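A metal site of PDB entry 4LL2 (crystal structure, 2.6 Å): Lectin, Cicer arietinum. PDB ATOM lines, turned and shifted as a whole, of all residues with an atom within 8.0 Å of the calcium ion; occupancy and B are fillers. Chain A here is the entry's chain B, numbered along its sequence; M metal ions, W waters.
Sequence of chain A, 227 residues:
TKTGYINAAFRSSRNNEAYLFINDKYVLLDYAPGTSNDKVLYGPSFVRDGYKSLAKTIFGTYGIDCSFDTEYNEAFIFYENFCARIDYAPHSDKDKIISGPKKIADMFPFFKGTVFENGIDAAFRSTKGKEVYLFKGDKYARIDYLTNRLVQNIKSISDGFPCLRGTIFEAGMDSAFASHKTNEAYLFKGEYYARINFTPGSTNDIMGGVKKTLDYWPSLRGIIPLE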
ATOM      1  N   TYR A   5     -19.405  20.074   5.892  1.00  0.00           N
ATOM      2  CA  TYR A   5     -18.026  20.051   5.404  1.00  0.00           C
ATOM      3  C   TYR A   5     -17.416  18.683   5.152  1.00  0.00           C
ATOM      4  O   TYR A   5     -18.098  17.735   5.197  1.00  0.00           O
ATOM      5  CB  TYR A   5     -17.158  20.848   6.338  1.00  0.00           C
ATOM      6  CG  TYR A   5     -17.494  22.296   6.343  1.00  0.00           C
ATOM      7  CD1 TYR A   5     -18.242  22.830   7.347  1.00  0.00           C
ATOM      8  CD2 TYR A   5     -17.090  23.132   5.317  1.00  0.00           C
ATOM      9  CE1 TYR A   5     -18.566  24.140   7.365  1.00  0.00           C
ATOM     10  CE2 TYR A   5     -17.400  24.426   5.332  1.00  0.00           C
ATOM     11  CZ  TYR A   5     -18.139  24.931   6.377  1.00  0.00           C
ATOM     12  OH  TYR A   5     -18.480  26.240   6.452  1.00  0.00           O
ATOM     13  N   ILE A   6     -16.140  18.583   4.861  1.00  0.00           N
ATOM     14  CA  ILE A   6     -15.516  17.286   4.638  1.00  0.00           C
ATOM     15  C   ILE A   6     -15.430  16.450   5.897  1.00  0.00           C
ATOM     16  O   ILE A   6     -14.944  16.879   6.888  1.00  0.00           O
ATOM     17  CB  ILE A   6     -14.142  17.440   3.972  1.00  0.00           C
ATOM     18  CG1 ILE A   6     -14.292  18.214   2.695  1.00  0.00           C
ATOM     19  CG2 ILE A   6     -13.537  16.119   3.657  1.00  0.00           C
ATOM     20  CD1 ILE A   6     -13.065  18.547   2.053  1.00  0.00           C
ATOM     21  N   ASN A   7     -15.933  15.235   5.866  1.00  0.00           N
ATOM     22  CA  ASN A   7     -15.951  14.457   7.063  1.00  0.00           C
ATOM     23  C   ASN A   7     -14.905  13.384   7.147  1.00  0.00           C
ATOM     24  O   ASN A   7     -14.565  12.929   8.186  1.00  0.00           O
ATOM     25  CB  ASN A   7     -17.354  13.917   7.356  1.00  0.00           C
ATOM     26  CG  ASN A   7     -17.619  13.816   8.786  1.00  0.00           C
ATOM     27  OD1 ASN A   7     -16.778  14.098   9.583  1.00  0.00           O
ATOM     28  ND2 ASN A   7     -18.764  13.378   9.127  1.00  0.00           N
ATOM     29  N   ALA A   8     -14.394  13.001   6.025  1.00  0.00           N
ATOM     30  CA  ALA A   8     -13.423  11.904   5.950  1.00  0.00           C
ATOM     31  C   ALA A   8     -12.716  11.925   4.603  1.00  0.00           C
ATOM     32  O   ALA A   8     -13.165  12.594   3.675  1.00  0.00           O
ATOM     33  CB  ALA A   8     -14.178  10.572   6.103  1.00  0.00           C
ATOM     34  N   ALA A   9     -11.606  11.211   4.501  1.00  0.00           N
ATOM     35  CA  ALA A   9     -10.854  11.137   3.251  1.00  0.00           C
ATOM     36  C   ALA A   9      -9.734  10.111   3.358  1.00  0.00           C
ATOM     37  O   ALA A   9      -9.378   9.713   4.451  1.00  0.00           O
ATOM     38  CB  ALA A   9     -10.236  12.511   2.927  1.00  0.00           C
ATOM     39  N   PHE A  21     -15.170  12.666   1.678  1.00  0.00           N
ATOM     40  CA  PHE A  21     -16.505  12.374   2.096  1.00  0.00           C
ATOM     41  C   PHE A  21     -17.213  13.533   2.739  1.00  0.00           C
ATOM     42  O   PHE A  21     -16.716  14.152   3.589  1.00  0.00           O
ATOM     43  CB  PHE A  21     -16.470  11.127   2.954  1.00  0.00           C
ATOM     44  CG  PHE A  21     -15.978   9.979   2.222  1.00  0.00           C
ATOM     45  CD1 PHE A  21     -16.786   9.267   1.431  1.00  0.00           C
ATOM     46  CD2 PHE A  21     -14.665   9.689   2.211  1.00  0.00           C
ATOM     47  CE1 PHE A  21     -16.321   8.299   0.717  1.00  0.00           C
ATOM     48  CE2 PHE A  21     -14.231   8.705   1.509  1.00  0.00           C
ATOM     49  CZ  PHE A  21     -15.048   8.010   0.745  1.00  0.00           C
ATOM     50  N   ILE A  64     -19.599   8.438   5.639  1.00  0.00           N
ATOM     51  CA  ILE A  64     -18.340   8.115   6.232  1.00  0.00           C
ATOM     52  C   ILE A  64     -17.803   9.313   7.009  1.00  0.00           C
ATOM     53  O   ILE A  64     -17.681  10.352   6.472  1.00  0.00           O
ATOM     54  CB  ILE A  64     -17.409   7.486   5.130  1.00  0.00           C
ATOM     55  CG1 ILE A  64     -17.793   6.052   4.926  1.00  0.00           C
ATOM     56  CG2 ILE A  64     -16.016   7.455   5.476  1.00  0.00           C
ATOM     57  CD1 ILE A  64     -18.105   5.732   3.643  1.00  0.00           C
ATOM     58  N   ASP A  65     -17.561   9.135   8.298  1.00  0.00           N
ATOM     59  CA  ASP A  65     -17.123  10.205   9.171  1.00  0.00           C
ATOM     60  C   ASP A  65     -15.666  10.201   9.540  1.00  0.00           C
ATOM     61  O   ASP A  65     -15.179  11.137  10.126  1.00  0.00           O
ATOM     62  CB  ASP A  65     -18.000  10.350  10.393  1.00  0.00           C
ATOM     63  CG  ASP A  65     -18.025   9.174  11.304  1.00  0.00           C
ATOM     64  OD1 ASP A  65     -17.163   8.370  11.352  1.00  0.00           O
ATOM     65  OD2 ASP A  65     -18.921   9.092  12.059  1.00  0.00           O
ATOM     66  N   CYS A  66     -14.975   9.181   9.112  1.00  0.00           N
ATOM     67  CA  CYS A  66     -13.529   9.062   9.340  1.00  0.00           C
ATOM     68  C   CYS A  66     -13.046   7.956   8.445  1.00  0.00           C
ATOM     69  O   CYS A  66     -13.824   7.078   8.070  1.00  0.00           O
ATOM     70  CB  CYS A  66     -13.181   8.732  10.801  1.00  0.00           C
ATOM     71  SG  CYS A  66     -11.376   8.465  10.956  1.00  0.00           S
ATOM     72  N   SER A  67     -11.757   7.974   8.111  1.00  0.00           N
ATOM     73  CA  SER A  67     -11.187   6.948   7.241  1.00  0.00           C
ATOM     74  C   SER A  67      -9.681   7.111   6.976  1.00  0.00           C
ATOM     75  O   SER A  67      -9.110   8.132   7.323  1.00  0.00           O
ATOM     76  CB  SER A  67     -11.890   6.988   5.891  1.00  0.00           C
ATOM     77  OG  SER A  67     -11.619   8.216   5.237  1.00  0.00           O
ATOM     78  N   PHE A  78     -15.258   4.710   8.608  1.00  0.00           N
ATOM     79  CA  PHE A  78     -15.903   4.768   9.893  1.00  0.00           C
ATOM     80  C   PHE A  78     -17.244   5.468   9.804  1.00  0.00           C
ATOM     81  O   PHE A  78     -17.484   6.247   8.936  1.00  0.00           O
ATOM     82  CB  PHE A  78     -14.987   5.412  10.933  1.00  0.00           C
ATOM     83  CG  PHE A  78     -13.732   4.673  11.188  1.00  0.00           C
ATOM     84  CD1 PHE A  78     -13.614   3.879  12.280  1.00  0.00           C
ATOM     85  CD2 PHE A  78     -12.653   4.827  10.379  1.00  0.00           C
ATOM     86  CE1 PHE A  78     -12.487   3.247  12.511  1.00  0.00           C
ATOM     87  CE2 PHE A  78     -11.580   4.199  10.609  1.00  0.00           C
ATOM     88  CZ  PHE A  78     -11.488   3.400  11.670  1.00  0.00           C
ATOM     89  N   ILE A 120     -14.291   8.181  15.899  1.00  0.00           N
ATOM     90  CA  ILE A 120     -13.028   8.779  15.573  1.00  0.00           C
ATOM     91  C   ILE A 120     -13.256   9.911  14.619  1.00  0.00           C
ATOM     92  O   ILE A 120     -13.952   9.767  13.678  1.00  0.00           O
ATOM     93  CB  ILE A 120     -12.066   7.788  14.870  1.00  0.00           C
ATOM     94  CG1 ILE A 120     -11.770   6.579  15.710  1.00  0.00           C
ATOM     95  CG2 ILE A 120     -10.774   8.444  14.516  1.00  0.00           C
ATOM     96  CD1 ILE A 120     -12.625   5.508  15.483  1.00  0.00           C
ATOM     97  N   ASP A 121     -12.687  11.065  14.893  1.00  0.00           N
ATOM     98  CA  ASP A 121     -12.804  12.240  14.022  1.00  0.00           C
ATOM     99  C   ASP A 121     -12.142  12.218  12.673  1.00  0.00           C
ATOM    100  O   ASP A 121     -12.683  12.627  11.689  1.00  0.00           O
ATOM    101  CB  ASP A 121     -12.349  13.478  14.750  1.00  0.00           C
ATOM    102  CG  ASP A 121     -13.213  13.843  15.838  1.00  0.00           C
ATOM    103  OD1 ASP A 121     -14.312  13.438  15.813  1.00  0.00           O
ATOM    104  OD2 ASP A 121     -12.824  14.508  16.757  1.00  0.00           O
ATOM    105  N   ALA A 122     -10.941  11.745  12.642  1.00  0.00           N
ATOM    106  CA  ALA A 122     -10.179  11.762  11.383  1.00  0.00           C
ATOM    107  C   ALA A 122      -8.900  10.958  11.471  1.00  0.00           C
ATOM    108  O   ALA A 122      -8.428  10.662  12.565  1.00  0.00           O
ATOM    109  CB  ALA A 122      -9.844  13.212  11.020  1.00  0.00           C
ATOM    110  N   ALA A 123      -8.330  10.612  10.314  1.00  0.00           N
ATOM    111  CA  ALA A 123      -7.108   9.835  10.310  1.00  0.00           C
ATOM    112  C   ALA A 123      -6.328   9.990   9.019  1.00  0.00           C
ATOM    113  O   ALA A 123      -6.837  10.523   8.041  1.00  0.00           O
ATOM    114  CB  ALA A 123      -7.471   8.356  10.491  1.00  0.00           C
ATOM    115  N   PHE A 135      -7.405  10.735  15.142  1.00  0.00           N
ATOM    116  CA  PHE A 135      -7.779  11.857  16.025  1.00  0.00           C
ATOM    117  C   PHE A 135      -9.209  11.850  16.583  1.00  0.00           C
ATOM    118  O   PHE A 135     -10.150  11.448  15.903  1.00  0.00           O
ATOM    119  CB  PHE A 135      -7.581  13.161  15.243  1.00  0.00           C
ATOM    120  CG  PHE A 135      -6.231  13.294  14.625  1.00  0.00           C
ATOM    121  CD1 PHE A 135      -5.222  13.963  15.296  1.00  0.00           C
ATOM    122  CD2 PHE A 135      -5.948  12.755  13.365  1.00  0.00           C
ATOM    123  CE1 PHE A 135      -3.941  14.091  14.748  1.00  0.00           C
ATOM    124  CE2 PHE A 135      -4.671  12.876  12.804  1.00  0.00           C
ATOM    125  CZ  PHE A 135      -3.663  13.553  13.497  1.00  0.00           C
ATOM    126  N   MET A 173      -9.948  17.809  14.746  1.00  0.00           N
ATOM    127  CA  MET A 173      -9.904  17.883  13.295  1.00  0.00           C
ATOM    128  C   MET A 173     -10.996  17.085  12.628  1.00  0.00           C
ATOM    129  O   MET A 173     -11.105  15.879  12.823  1.00  0.00           O
ATOM    130  CB  MET A 173      -8.579  17.401  12.792  1.00  0.00           C
ATOM    131  CG  MET A 173      -7.434  18.142  13.390  1.00  0.00           C
ATOM    132  SD  MET A 173      -6.057  17.044  13.308  1.00  0.00           S
ATOM    133  CE  MET A 173      -6.316  16.339  11.641  1.00  0.00           C
ATOM    134  N   ASP A 174     -11.794  17.781  11.837  1.00  0.00           N
ATOM    135  CA  ASP A 174     -12.905  17.172  11.137  1.00  0.00           C
ATOM    136  C   ASP A 174     -12.511  16.083  10.149  1.00  0.00           C
ATOM    137  O   ASP A 174     -13.236  15.122   9.981  1.00  0.00           O
ATOM    138  CB  ASP A 174     -13.674  18.268  10.380  1.00  0.00           C
ATOM    139  CG  ASP A 174     -14.557  19.099  11.278  1.00  0.00           C
ATOM    140  OD1 ASP A 174     -15.042  20.164  10.827  1.00  0.00           O
ATOM    141  OD2 ASP A 174     -14.763  18.690  12.447  1.00  0.00           O
ATOM    142  N   SER A 175     -11.348  16.227   9.517  1.00  0.00           N
ATOM    143  CA  SER A 175     -11.009  15.287   8.455  1.00  0.00           C
ATOM    144  C   SER A 175      -9.536  15.365   8.002  1.00  0.00           C
ATOM    145  O   SER A 175      -8.886  16.384   8.185  1.00  0.00           O
ATOM    146  CB  SER A 175     -11.932  15.688   7.292  1.00  0.00           C
ATOM    147  OG  SER A 175     -11.780  14.870   6.147  1.00  0.00           O
ATOM    148  N   ALA A 176      -9.021  14.302   7.409  1.00  0.00           N
ATOM    149  CA  ALA A 176      -7.650  14.324   6.922  1.00  0.00           C
ATOM    150  C   ALA A 176      -7.301  13.229   5.928  1.00  0.00           C
ATOM    151  O   ALA A 176      -8.063  12.306   5.697  1.00  0.00           O
ATOM    152  CB  ALA A 176      -6.683  14.206   8.119  1.00  0.00           C
ATOM    153  N   PHE A 188      -8.517  19.071   7.669  1.00  0.00           N
ATOM    154  CA  PHE A 188      -9.641  19.936   7.386  1.00  0.00           C
ATOM    155  C   PHE A 188     -10.477  20.225   8.616  1.00  0.00           C
ATOM    156  O   PHE A 188     -10.574  19.392   9.528  1.00  0.00           O
ATOM    157  CB  PHE A 188     -10.555  19.325   6.299  1.00  0.00           C
ATOM    158  CG  PHE A 188      -9.857  19.112   4.980  1.00  0.00           C
ATOM    159  CD1 PHE A 188      -9.056  17.992   4.751  1.00  0.00           C
ATOM    160  CD2 PHE A 188      -9.980  20.055   3.953  1.00  0.00           C
ATOM    161  CE1 PHE A 188      -8.396  17.814   3.554  1.00  0.00           C
ATOM    162  CE2 PHE A 188      -9.318  19.883   2.733  1.00  0.00           C
ATOM    163  CZ  PHE A 188      -8.529  18.767   2.532  1.00  0.00           C
HETATM  164 CA    CA M   1     -14.857  13.473  10.662  1.00  0.00          CA
HETATM  165  O   HOH W   1     -15.994  12.164  12.866  1.00  0.00           O
HETATM  166  O   HOH W   2     -15.411  15.444  12.782  1.00  0.00           O
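The calcium ion is bound by the side-chain amide oxygen (OD1) of Asn 7 (2.3 Å), the backbone carbonyl oxygen (O) of Asp 174 (2.4 Å), the backbone carbonyl oxygen (O) of Asp 65 (2.4 Å), the backbone carbonyl oxygen (O) of Asp 121 (2.5 Å), the backbone carbonyl oxygen (O) of Asn 7 (2.6 Å) and water W1 (2.8 Å).
The calcium ion has six donor atoms within binding distance.
Slightly farther from the calcium ion lies water W2 (2.9 Å).
The backbone NH (N) of Asn 7 is in hydrogen-bond range of the backbone carbonyl oxygen (O) of Phe 21, 2.6 Å away.
The backbone NH (N) of Asp 174 is in hydrogen-bond range of the backbone carbonyl oxygen (O) of Phe 188 (3.1 Å).
The backbone carbonyl oxygen of Phe 78 lies within hydrogen-bond range of the backbone NH of Asp 65 (3.0 Å).
The backbone NH (N) of Asp 121 is in hydrogen-bond range of the backbone carbonyl oxygen (O) of Phe 135, at 2.8 Å.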
